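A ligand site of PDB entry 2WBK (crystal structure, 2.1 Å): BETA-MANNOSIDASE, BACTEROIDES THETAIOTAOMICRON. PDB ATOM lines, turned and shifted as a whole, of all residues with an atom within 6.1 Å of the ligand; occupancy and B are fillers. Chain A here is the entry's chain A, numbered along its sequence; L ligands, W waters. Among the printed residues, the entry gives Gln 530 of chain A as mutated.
The side-chain carboxylate of Asp 174 lies within hydrogen-bond range of an oxygen (O8) of the ligand, at 2.6 Å. An oxygen (O8) of the ligand lies within hydrogen-bond range of the indole nitrogen (NE1) of Trp 175 (2.9 Å). OH of Tyr 512 is in hydrogen-bond range of O9 of the ligand (2.6 Å). The side-chain amide nitrogen (ND2) of Asn 153 is in hydrogen-bond range of an oxygen (O2) of the ligand, 3.2 Å away. The side-chain sulfur of Cys 399 sits at hydrogen-bond distance from an oxygen (O1) of the ligand (3.5 Å). The indole nitrogen (NE1) of Trp 173 sits at hydrogen-bond distance from an oxygen (O7) of the ligand.
The backbone carbonyl oxygen of Asn 436 lies within hydrogen-bond range of the backbone NH of Cys 399. The side-chain amide oxygen of Asn 436 lies within hydrogen-bond range of the guanidinium group of Arg 368. OE1 of Gln 621 sits at hydrogen-bond distance from NE1 of Trp 620 (2.9 Å). O of Trp 631 is in hydrogen-bond range of N of Gln 621, at 3.2 Å. OD1 of Asp 174 lies close to NE1 of Trp 175 (3.4 Å). NE1 of Trp 508 is in hydrogen-bond range of OE1 of Gln 530, 3.0 Å away. The side-chain amide oxygen (OE1) of Gln 530 lies within hydrogen-bond range of a ring nitrogen (ND1) of His 506. OD1 of Asn 436 sits at hydrogen-bond distance from NE2 of Gln 530 (3.0 Å).
The indole nitrogen (NE1) of Trp 370 sits close to a fluorine (F1) of the ligand (3.2 Å). The side-chain amide nitrogen of Asn 436 lies close to a fluorine (F1) of the ligand, at 2.7 Å. The side-chain carboxylate of Glu 437 lies close to an oxygen (O5) of the ligand, at 3.1 Å. A fluorine (F1) of the ligand sits close to the side-chain amide nitrogen of Gln 530 (3.1 Å). CH2 of Trp 445 touches C2 of the ligand, at 3.6 Å. CZ2 of Trp 508 touches O6 of the ligand, 3.2 Å away. Trp 620 touches the ligand (NE1 to C11, 3.3 Å). Trp 631 touches the ligand (CZ2 to C12, 3.6 Å). Of the 21 residues printed, 14 come within 4 Å of the ligand.
Water W1 lies within hydrogen-bond range of an oxygen (O2) of the ligand (2.9 Å), the side-chain hydroxyl of Tyr 512 (3.2 Å) and the side-chain carboxylate of Asp 174 (3.2 Å). Water W2 lies within hydrogen-bond range of an oxygen (O4) of the ligand (2.8 Å), the indole nitrogen of Trp 494 (2.9 Å) and the indole nitrogen of Trp 445 (3.5 Å).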
ATOM      1  N   ASN A 153      -6.188   2.320 -29.492  1.00  0.00           N
ATOM      2  CA  ASN A 153      -6.100   3.397 -28.517  1.00  0.00           C
ATOM      3  C   ASN A 153      -4.819   3.348 -27.678  1.00  0.00           C
ATOM      4  O   ASN A 153      -4.499   4.321 -26.978  1.00  0.00           O
ATOM      5  CB  ASN A 153      -7.337   3.414 -27.607  1.00  0.00           C
ATOM      6  CG  ASN A 153      -8.575   3.945 -28.322  1.00  0.00           C
ATOM      7  OD1 ASN A 153      -8.647   5.145 -28.656  1.00  0.00           O
ATOM      8  ND2 ASN A 153      -9.533   3.034 -28.639  1.00  0.00           N
ATOM      9  N   TRP A 173      -5.739   7.369 -25.391  1.00  0.00           N
ATOM     10  CA  TRP A 173      -7.104   7.044 -25.858  1.00  0.00           C
ATOM     11  C   TRP A 173      -7.484   8.119 -26.881  1.00  0.00           C
ATOM     12  O   TRP A 173      -6.706   9.097 -27.083  1.00  0.00           O
ATOM     13  CB  TRP A 173      -8.142   6.967 -24.711  1.00  0.00           C
ATOM     14  CG  TRP A 173      -9.185   5.944 -25.012  1.00  0.00           C
ATOM     15  CD1 TRP A 173     -10.401   6.162 -25.592  1.00  0.00           C
ATOM     16  CD2 TRP A 173      -9.106   4.517 -24.798  1.00  0.00           C
ATOM     17  NE1 TRP A 173     -11.050   4.983 -25.799  1.00  0.00           N
ATOM     18  CE2 TRP A 173     -10.291   3.956 -25.284  1.00  0.00           C
ATOM     19  CE3 TRP A 173      -8.137   3.666 -24.249  1.00  0.00           C
ATOM     20  CZ2 TRP A 173     -10.540   2.559 -25.263  1.00  0.00           C
ATOM     21  CZ3 TRP A 173      -8.384   2.268 -24.218  1.00  0.00           C
ATOM     22  CH2 TRP A 173      -9.576   1.743 -24.707  1.00  0.00           C
ATOM     23  N   ASP A 174      -8.645   7.979 -27.529  1.00  0.00           N
ATOM     24  CA  ASP A 174      -8.991   8.971 -28.585  1.00  0.00           C
ATOM     25  C   ASP A 174      -9.521  10.294 -28.059  1.00  0.00           C
ATOM     26  O   ASP A 174     -10.073  11.088 -28.830  1.00  0.00           O
ATOM     27  CB  ASP A 174      -9.993   8.368 -29.626  1.00  0.00           C
ATOM     28  CG  ASP A 174     -11.356   7.943 -28.991  1.00  0.00           C
ATOM     29  OD1 ASP A 174     -11.617   8.193 -27.778  1.00  0.00           O
ATOM     30  OD2 ASP A 174     -12.199   7.395 -29.762  1.00  0.00           O
ATOM     31  N   TRP A 175      -9.474  10.493 -26.757  1.00  0.00           N
ATOM     32  CA  TRP A 175      -9.687  11.826 -26.167  1.00  0.00           C
ATOM     33  C   TRP A 175      -8.589  11.950 -25.118  1.00  0.00           C
ATOM     34  O   TRP A 175      -8.635  12.824 -24.223  1.00  0.00           O
ATOM     35  CB  TRP A 175     -11.069  11.898 -25.452  1.00  0.00           C
ATOM     36  CG  TRP A 175     -11.472  10.577 -24.825  1.00  0.00           C
ATOM     37  CD1 TRP A 175     -12.441   9.721 -25.276  1.00  0.00           C
ATOM     38  CD2 TRP A 175     -10.907   9.955 -23.635  1.00  0.00           C
ATOM     39  NE1 TRP A 175     -12.501   8.615 -24.477  1.00  0.00           N
ATOM     40  CE2 TRP A 175     -11.576   8.726 -23.469  1.00  0.00           C
ATOM     41  CE3 TRP A 175      -9.886  10.318 -22.729  1.00  0.00           C
ATOM     42  CZ2 TRP A 175     -11.266   7.819 -22.391  1.00  0.00           C
ATOM     43  CZ3 TRP A 175      -9.578   9.426 -21.659  1.00  0.00           C
ATOM     44  CH2 TRP A 175     -10.283   8.174 -21.518  1.00  0.00           C
ATOM     45  N   ARG A 368     -22.270   5.136 -15.816  1.00  0.00           N
ATOM     46  CA  ARG A 368     -21.518   3.939 -16.151  1.00  0.00           C
ATOM     47  C   ARG A 368     -20.011   4.217 -16.031  1.00  0.00           C
ATOM     48  O   ARG A 368     -19.491   5.163 -16.682  1.00  0.00           O
ATOM     49  CB  ARG A 368     -21.872   3.523 -17.573  1.00  0.00           C
ATOM     50  CG  ARG A 368     -21.059   2.370 -18.094  1.00  0.00           C
ATOM     51  CD  ARG A 368     -21.452   1.953 -19.495  1.00  0.00           C
ATOM     52  NE  ARG A 368     -20.531   0.931 -19.921  1.00  0.00           N
ATOM     53  CZ  ARG A 368     -20.094   0.769 -21.166  1.00  0.00           C
ATOM     54  NH1 ARG A 368     -20.585   1.530 -22.145  1.00  0.00           N
ATOM     55  NH2 ARG A 368     -19.192  -0.184 -21.419  1.00  0.00           N
ATOM     56  N   TRP A 370     -16.896   3.301 -17.294  1.00  0.00           N
ATOM     57  CA  TRP A 370     -16.457   2.629 -18.522  1.00  0.00           C
ATOM     58  C   TRP A 370     -15.110   1.919 -18.322  1.00  0.00           C
ATOM     59  O   TRP A 370     -14.225   2.434 -17.587  1.00  0.00           O
ATOM     60  CB  TRP A 370     -16.406   3.702 -19.658  1.00  0.00           C
ATOM     61  CG  TRP A 370     -15.560   3.423 -20.839  1.00  0.00           C
ATOM     62  CD1 TRP A 370     -15.936   2.762 -21.969  1.00  0.00           C
ATOM     63  CD2 TRP A 370     -14.210   3.924 -21.084  1.00  0.00           C
ATOM     64  NE1 TRP A 370     -14.884   2.764 -22.890  1.00  0.00           N
ATOM     65  CE2 TRP A 370     -13.824   3.462 -22.361  1.00  0.00           C
ATOM     66  CE3 TRP A 370     -13.276   4.625 -20.313  1.00  0.00           C
ATOM     67  CZ2 TRP A 370     -12.558   3.708 -22.904  1.00  0.00           C
ATOM     68  CZ3 TRP A 370     -12.008   4.870 -20.846  1.00  0.00           C
ATOM     69  CH2 TRP A 370     -11.671   4.398 -22.143  1.00  0.00           C
ATOM     70  N   ALA A 398     -11.429  -2.902 -22.533  1.00  0.00           N
ATOM     71  CA  ALA A 398     -12.089  -2.052 -23.518  1.00  0.00           C
ATOM     72  C   ALA A 398     -11.504  -2.049 -24.881  1.00  0.00           C
ATOM     73  O   ALA A 398     -10.305  -1.790 -25.071  1.00  0.00           O
ATOM     74  CB  ALA A 398     -12.214  -0.619 -23.019  1.00  0.00           C
ATOM     75  N   CYS A 399     -12.387  -2.275 -25.855  1.00  0.00           N
ATOM     76  CA  CYS A 399     -12.097  -1.983 -27.275  1.00  0.00           C
ATOM     77  C   CYS A 399     -11.083  -2.864 -27.996  1.00  0.00           C
ATOM     78  O   CYS A 399     -10.715  -2.592 -29.147  1.00  0.00           O
ATOM     79  CB  CYS A 399     -11.721  -0.485 -27.408  1.00  0.00           C
ATOM     80  SG  CYS A 399     -13.109   0.519 -26.865  1.00  0.00           S
ATOM     81  N   ASN A 436     -16.206  -3.282 -22.454  1.00  0.00           N
ATOM     82  CA  ASN A 436     -16.755  -2.356 -23.414  1.00  0.00           C
ATOM     83  C   ASN A 436     -16.394  -2.713 -24.878  1.00  0.00           C
ATOM     84  O   ASN A 436     -15.218  -2.621 -25.306  1.00  0.00           O
ATOM     85  CB  ASN A 436     -16.267  -0.909 -23.114  1.00  0.00           C
ATOM     86  CG  ASN A 436     -16.790   0.112 -24.151  1.00  0.00           C
ATOM     87  OD1 ASN A 436     -17.948   0.567 -24.083  1.00  0.00           O
ATOM     88  ND2 ASN A 436     -15.934   0.489 -25.121  1.00  0.00           N
ATOM     89  N   GLU A 437     -17.426  -3.104 -25.629  1.00  0.00           N
ATOM     90  CA  GLU A 437     -17.348  -3.193 -27.103  1.00  0.00           C
ATOM     91  C   GLU A 437     -16.470  -4.315 -27.626  1.00  0.00           C
ATOM     92  O   GLU A 437     -16.129  -4.324 -28.803  1.00  0.00           O
ATOM     93  CB  GLU A 437     -16.890  -1.839 -27.687  1.00  0.00           C
ATOM     94  CG  GLU A 437     -18.019  -0.742 -27.614  1.00  0.00           C
ATOM     95  CD  GLU A 437     -17.722   0.579 -28.307  1.00  0.00           C
ATOM     96  OE1 GLU A 437     -16.603   0.740 -28.793  1.00  0.00           O
ATOM     97  OE2 GLU A 437     -18.593   1.477 -28.352  1.00  0.00           O
ATOM     98  N   GLU A 440     -18.248  -6.585 -30.012  1.00  0.00           N
ATOM     99  CA  GLU A 440     -18.437  -5.776 -31.209  1.00  0.00           C
ATOM    100  C   GLU A 440     -17.191  -5.682 -32.093  1.00  0.00           C
ATOM    101  O   GLU A 440     -17.254  -5.872 -33.348  1.00  0.00           O
ATOM    102  CB  GLU A 440     -19.010  -4.406 -30.905  1.00  0.00           C
ATOM    103  CG  GLU A 440     -19.181  -3.533 -32.149  1.00  0.00           C
ATOM    104  CD  GLU A 440     -20.129  -2.390 -31.918  1.00  0.00           C
ATOM    105  OE1 GLU A 440     -20.111  -1.794 -30.841  1.00  0.00           O
ATOM    106  OE2 GLU A 440     -20.938  -2.072 -32.819  1.00  0.00           O
ATOM    107  N   TRP A 445     -15.294  -5.035 -36.520  1.00  0.00           N
ATOM    108  CA  TRP A 445     -14.316  -3.983 -36.773  1.00  0.00           C
ATOM    109  C   TRP A 445     -13.235  -4.400 -37.775  1.00  0.00           C
ATOM    110  O   TRP A 445     -12.271  -3.647 -37.976  1.00  0.00           O
ATOM    111  CB  TRP A 445     -13.700  -3.451 -35.475  1.00  0.00           C
ATOM    112  CG  TRP A 445     -14.661  -2.694 -34.599  1.00  0.00           C
ATOM    113  CD1 TRP A 445     -16.002  -2.461 -34.821  1.00  0.00           C
ATOM    114  CD2 TRP A 445     -14.377  -2.121 -33.313  1.00  0.00           C
ATOM    115  NE1 TRP A 445     -16.550  -1.767 -33.759  1.00  0.00           N
ATOM    116  CE2 TRP A 445     -15.575  -1.527 -32.828  1.00  0.00           C
ATOM    117  CE3 TRP A 445     -13.208  -2.044 -32.519  1.00  0.00           C
ATOM    118  CZ2 TRP A 445     -15.645  -0.877 -31.584  1.00  0.00           C
ATOM    119  CZ3 TRP A 445     -13.289  -1.384 -31.292  1.00  0.00           C
ATOM    120  CH2 TRP A 445     -14.480  -0.816 -30.834  1.00  0.00           C
ATOM    121  N   TRP A 494     -24.789  -0.809 -34.320  1.00  0.00           N
ATOM    122  CA  TRP A 494     -25.412   0.356 -34.912  1.00  0.00           C
ATOM    123  C   TRP A 494     -25.556   0.249 -36.426  1.00  0.00           C
ATOM    124  O   TRP A 494     -26.357   0.979 -36.995  1.00  0.00           O
ATOM    125  CB  TRP A 494     -24.661   1.651 -34.547  1.00  0.00           C
ATOM    126  CG  TRP A 494     -23.281   1.810 -35.070  1.00  0.00           C
ATOM    127  CD1 TRP A 494     -22.093   1.545 -34.396  1.00  0.00           C
ATOM    128  CD2 TRP A 494     -22.883   2.308 -36.373  1.00  0.00           C
ATOM    129  NE1 TRP A 494     -21.013   1.838 -35.207  1.00  0.00           N
ATOM    130  CE2 TRP A 494     -21.466   2.313 -36.407  1.00  0.00           C
ATOM    131  CE3 TRP A 494     -23.587   2.779 -37.497  1.00  0.00           C
ATOM    132  CZ2 TRP A 494     -20.744   2.754 -37.531  1.00  0.00           C
ATOM    133  CZ3 TRP A 494     -22.878   3.178 -38.613  1.00  0.00           C
ATOM    134  CH2 TRP A 494     -21.470   3.165 -38.627  1.00  0.00           C
ATOM    135  N   HIS A 506     -24.829   0.887 -28.603  1.00  0.00           N
ATOM    136  CA  HIS A 506     -23.935   2.028 -28.737  1.00  0.00           C
ATOM    137  C   HIS A 506     -24.225   2.555 -30.128  1.00  0.00           C
ATOM    138  O   HIS A 506     -23.671   2.027 -31.093  1.00  0.00           O
ATOM    139  CB  HIS A 506     -22.436   1.647 -28.600  1.00  0.00           C
ATOM    140  CG  HIS A 506     -22.071   1.093 -27.254  1.00  0.00           C
ATOM    141  ND1 HIS A 506     -20.758   0.971 -26.841  1.00  0.00           N
ATOM    142  CD2 HIS A 506     -22.837   0.612 -26.239  1.00  0.00           C
ATOM    143  CE1 HIS A 506     -20.750   0.427 -25.631  1.00  0.00           C
ATOM    144  NE2 HIS A 506     -21.988   0.220 -25.235  1.00  0.00           N
ATOM    145  N   TRP A 508     -23.383   4.518 -32.662  1.00  0.00           N
ATOM    146  CA  TRP A 508     -22.332   5.377 -33.151  1.00  0.00           C
ATOM    147  C   TRP A 508     -22.559   5.740 -34.624  1.00  0.00           C
ATOM    148  O   TRP A 508     -21.661   6.226 -35.307  1.00  0.00           O
ATOM    149  CB  TRP A 508     -20.921   4.772 -32.857  1.00  0.00           C
ATOM    150  CG  TRP A 508     -20.483   5.022 -31.461  1.00  0.00           C
ATOM    151  CD1 TRP A 508     -20.303   4.082 -30.459  1.00  0.00           C
ATOM    152  CD2 TRP A 508     -20.221   6.310 -30.845  1.00  0.00           C
ATOM    153  NE1 TRP A 508     -19.907   4.700 -29.279  1.00  0.00           N
ATOM    154  CE2 TRP A 508     -19.840   6.061 -29.488  1.00  0.00           C
ATOM    155  CE3 TRP A 508     -20.210   7.625 -31.318  1.00  0.00           C
ATOM    156  CZ2 TRP A 508     -19.480   7.073 -28.615  1.00  0.00           C
ATOM    157  CZ3 TRP A 508     -19.851   8.655 -30.421  1.00  0.00           C
ATOM    158  CH2 TRP A 508     -19.482   8.370 -29.108  1.00  0.00           C
ATOM    159  N   TRP A 511     -21.911  10.508 -35.578  1.00  0.00           N
ATOM    160  CA  TRP A 511     -20.451  10.545 -35.452  1.00  0.00           C
ATOM    161  C   TRP A 511     -19.838   9.523 -36.381  1.00  0.00           C
ATOM    162  O   TRP A 511     -19.655   9.828 -37.542  1.00  0.00           O
ATOM    163  CB  TRP A 511     -19.938  10.419 -33.996  1.00  0.00           C
ATOM    164  CG  TRP A 511     -18.526  10.793 -33.910  1.00  0.00           C
ATOM    165  CD1 TRP A 511     -17.444   9.948 -33.766  1.00  0.00           C
ATOM    166  CD2 TRP A 511     -17.981  12.132 -33.997  1.00  0.00           C
ATOM    167  NE1 TRP A 511     -16.270  10.695 -33.750  1.00  0.00           N
ATOM    168  CE2 TRP A 511     -16.579  12.025 -33.887  1.00  0.00           C
ATOM    169  CE3 TRP A 511     -18.552  13.397 -34.180  1.00  0.00           C
ATOM    170  CZ2 TRP A 511     -15.731  13.132 -33.972  1.00  0.00           C
ATOM    171  CZ3 TRP A 511     -17.719  14.509 -34.239  1.00  0.00           C
ATOM    172  CH2 TRP A 511     -16.313  14.367 -34.136  1.00  0.00           C
ATOM    173  N   TYR A 512     -19.578   8.301 -35.912  1.00  0.00           N
ATOM    174  CA  TYR A 512     -18.866   7.342 -36.775  1.00  0.00           C
ATOM    175  C   TYR A 512     -19.596   7.071 -38.109  1.00  0.00           C
ATOM    176  O   TYR A 512     -18.975   6.987 -39.160  1.00  0.00           O
ATOM    177  CB  TYR A 512     -18.613   6.017 -36.017  1.00  0.00           C
ATOM    178  CG  TYR A 512     -17.479   6.112 -35.024  1.00  0.00           C
ATOM    179  CD1 TYR A 512     -16.150   5.889 -35.404  1.00  0.00           C
ATOM    180  CD2 TYR A 512     -17.736   6.459 -33.693  1.00  0.00           C
ATOM    181  CE1 TYR A 512     -15.110   5.974 -34.461  1.00  0.00           C
ATOM    182  CE2 TYR A 512     -16.704   6.567 -32.755  1.00  0.00           C
ATOM    183  CZ  TYR A 512     -15.418   6.317 -33.128  1.00  0.00           C
ATOM    184  OH  TYR A 512     -14.436   6.423 -32.156  1.00  0.00           O
ATOM    185  N   GLN A 530     -24.509   3.900 -25.089  1.00  0.00           N
ATOM    186  CA  GLN A 530     -23.665   5.009 -25.549  1.00  0.00           C
ATOM    187  C   GLN A 530     -24.200   5.663 -26.826  1.00  0.00           C
ATOM    188  O   GLN A 530     -24.670   4.976 -27.778  1.00  0.00           O
ATOM    189  CB  GLN A 530     -22.216   4.569 -25.847  1.00  0.00           C
ATOM    190  CG  GLN A 530     -21.338   4.078 -24.698  1.00  0.00           C
ATOM    191  CD  GLN A 530     -19.904   3.819 -25.173  1.00  0.00           C
ATOM    192  OE1 GLN A 530     -19.595   3.958 -26.371  1.00  0.00           O
ATOM    193  NE2 GLN A 530     -19.041   3.374 -24.253  1.00  0.00           N
ATOM    194  N   TRP A 620     -22.122   9.385 -24.300  1.00  0.00           N
ATOM    195  CA  TRP A 620     -20.691   9.330 -24.221  1.00  0.00           C
ATOM    196  C   TRP A 620     -20.296  10.771 -24.524  1.00  0.00           C
ATOM    197  O   TRP A 620     -20.592  11.209 -25.624  1.00  0.00           O
ATOM    198  CB  TRP A 620     -20.101   8.425 -25.326  1.00  0.00           C
ATOM    199  CG  TRP A 620     -18.588   8.452 -25.193  1.00  0.00           C
ATOM    200  CD1 TRP A 620     -17.739   9.321 -25.785  1.00  0.00           C
ATOM    201  CD2 TRP A 620     -17.810   7.652 -24.315  1.00  0.00           C
ATOM    202  NE1 TRP A 620     -16.458   9.104 -25.347  1.00  0.00           N
ATOM    203  CE2 TRP A 620     -16.474   8.081 -24.442  1.00  0.00           C
ATOM    204  CE3 TRP A 620     -18.107   6.618 -23.423  1.00  0.00           C
ATOM    205  CZ2 TRP A 620     -15.431   7.509 -23.714  1.00  0.00           C
ATOM    206  CZ3 TRP A 620     -17.100   6.056 -22.694  1.00  0.00           C
ATOM    207  CH2 TRP A 620     -15.771   6.503 -22.847  1.00  0.00           C
ATOM    208  N   GLN A 621     -19.641  11.520 -23.621  1.00  0.00           N
ATOM    209  CA  GLN A 621     -19.102  11.037 -22.341  1.00  0.00           C
ATOM    210  C   GLN A 621     -19.358  12.170 -21.373  1.00  0.00           C
ATOM    211  O   GLN A 621     -19.583  13.343 -21.816  1.00  0.00           O
ATOM    212  CB  GLN A 621     -17.542  10.822 -22.456  1.00  0.00           C
ATOM    213  CG  GLN A 621     -16.673  12.151 -22.701  1.00  0.00           C
ATOM    214  CD  GLN A 621     -15.283  11.911 -23.402  1.00  0.00           C
ATOM    215  OE1 GLN A 621     -15.191  11.636 -24.616  1.00  0.00           O
ATOM    216  NE2 GLN A 621     -14.208  12.055 -22.637  1.00  0.00           N
ATOM    217  N   TRP A 631     -15.874  14.230 -26.543  1.00  0.00           N
ATOM    218  CA  TRP A 631     -17.322  14.081 -26.533  1.00  0.00           C
ATOM    219  C   TRP A 631     -17.956  14.520 -25.195  1.00  0.00           C
ATOM    220  O   TRP A 631     -19.145  14.353 -25.005  1.00  0.00           O
ATOM    221  CB  TRP A 631     -17.678  12.644 -26.804  1.00  0.00           C
ATOM    222  CG  TRP A 631     -17.181  12.143 -28.157  1.00  0.00           C
ATOM    223  CD1 TRP A 631     -17.957  11.932 -29.282  1.00  0.00           C
ATOM    224  CD2 TRP A 631     -15.847  11.700 -28.498  1.00  0.00           C
ATOM    225  NE1 TRP A 631     -17.169  11.427 -30.304  1.00  0.00           N
ATOM    226  CE2 TRP A 631     -15.882  11.264 -29.849  1.00  0.00           C
ATOM    227  CE3 TRP A 631     -14.641  11.610 -27.802  1.00  0.00           C
ATOM    228  CZ2 TRP A 631     -14.736  10.776 -30.514  1.00  0.00           C
ATOM    229  CZ3 TRP A 631     -13.514  11.143 -28.458  1.00  0.00           C
ATOM    230  CH2 TRP A 631     -13.577  10.708 -29.802  1.00  0.00           C
HETATM  231  O1  LIG L   1     -12.781   3.505 -28.568  1.00  0.00           O
HETATM  232  N1  LIG L   1     -13.134   2.842 -29.745  1.00  0.00           N
HETATM  233  O2  LIG L   1     -12.140   2.025 -30.242  1.00  0.00           O
HETATM  234  C1  LIG L   1     -14.372   2.961 -30.376  1.00  0.00           C
HETATM  235  C2  LIG L   1     -14.453   2.687 -31.744  1.00  0.00           C
HETATM  236  C3  LIG L   1     -15.648   2.765 -32.455  1.00  0.00           C
HETATM  237  N2  LIG L   1     -15.561   2.453 -33.767  1.00  0.00           N
HETATM  238  O3  LIG L   1     -14.256   2.393 -34.335  1.00  0.00           O
HETATM  239  O4  LIG L   1     -16.695   2.162 -34.581  1.00  0.00           O
HETATM  240  C4  LIG L   1     -16.846   3.145 -31.814  1.00  0.00           C
HETATM  241  C5  LIG L   1     -16.774   3.441 -30.451  1.00  0.00           C
HETATM  242  C6  LIG L   1     -15.559   3.345 -29.717  1.00  0.00           C
HETATM  243  O5  LIG L   1     -15.467   3.620 -28.363  1.00  0.00           O
HETATM  244  C7  LIG L   1     -16.543   4.311 -27.697  1.00  0.00           C
HETATM  245  O6  LIG L   1     -16.639   5.631 -28.214  1.00  0.00           O
HETATM  246  C8  LIG L   1     -16.194   4.357 -26.235  1.00  0.00           C
HETATM  247  F1  LIG L   1     -16.272   3.104 -25.714  1.00  0.00           F
HETATM  248  C9  LIG L   1     -14.779   5.003 -26.047  1.00  0.00           C
HETATM  249  O7  LIG L   1     -13.808   3.991 -26.201  1.00  0.00           O
HETATM  250  C10 LIG L   1     -14.540   6.082 -27.084  1.00  0.00           C
HETATM  251  O8  LIG L   1     -13.701   7.122 -26.614  1.00  0.00           O
HETATM  252  C11 LIG L   1     -15.867   6.703 -27.585  1.00  0.00           C
HETATM  253  C12 LIG L   1     -15.594   7.842 -28.665  1.00  0.00           C
HETATM  254  O9  LIG L   1     -14.905   7.255 -29.779  1.00  0.00           O
HETATM  255  O   HOH W   1     -11.946   4.641 -31.371  1.00  0.00           O
HETATM  256  O   HOH W   2     -18.867   0.822 -33.507  1.00  0.00           O
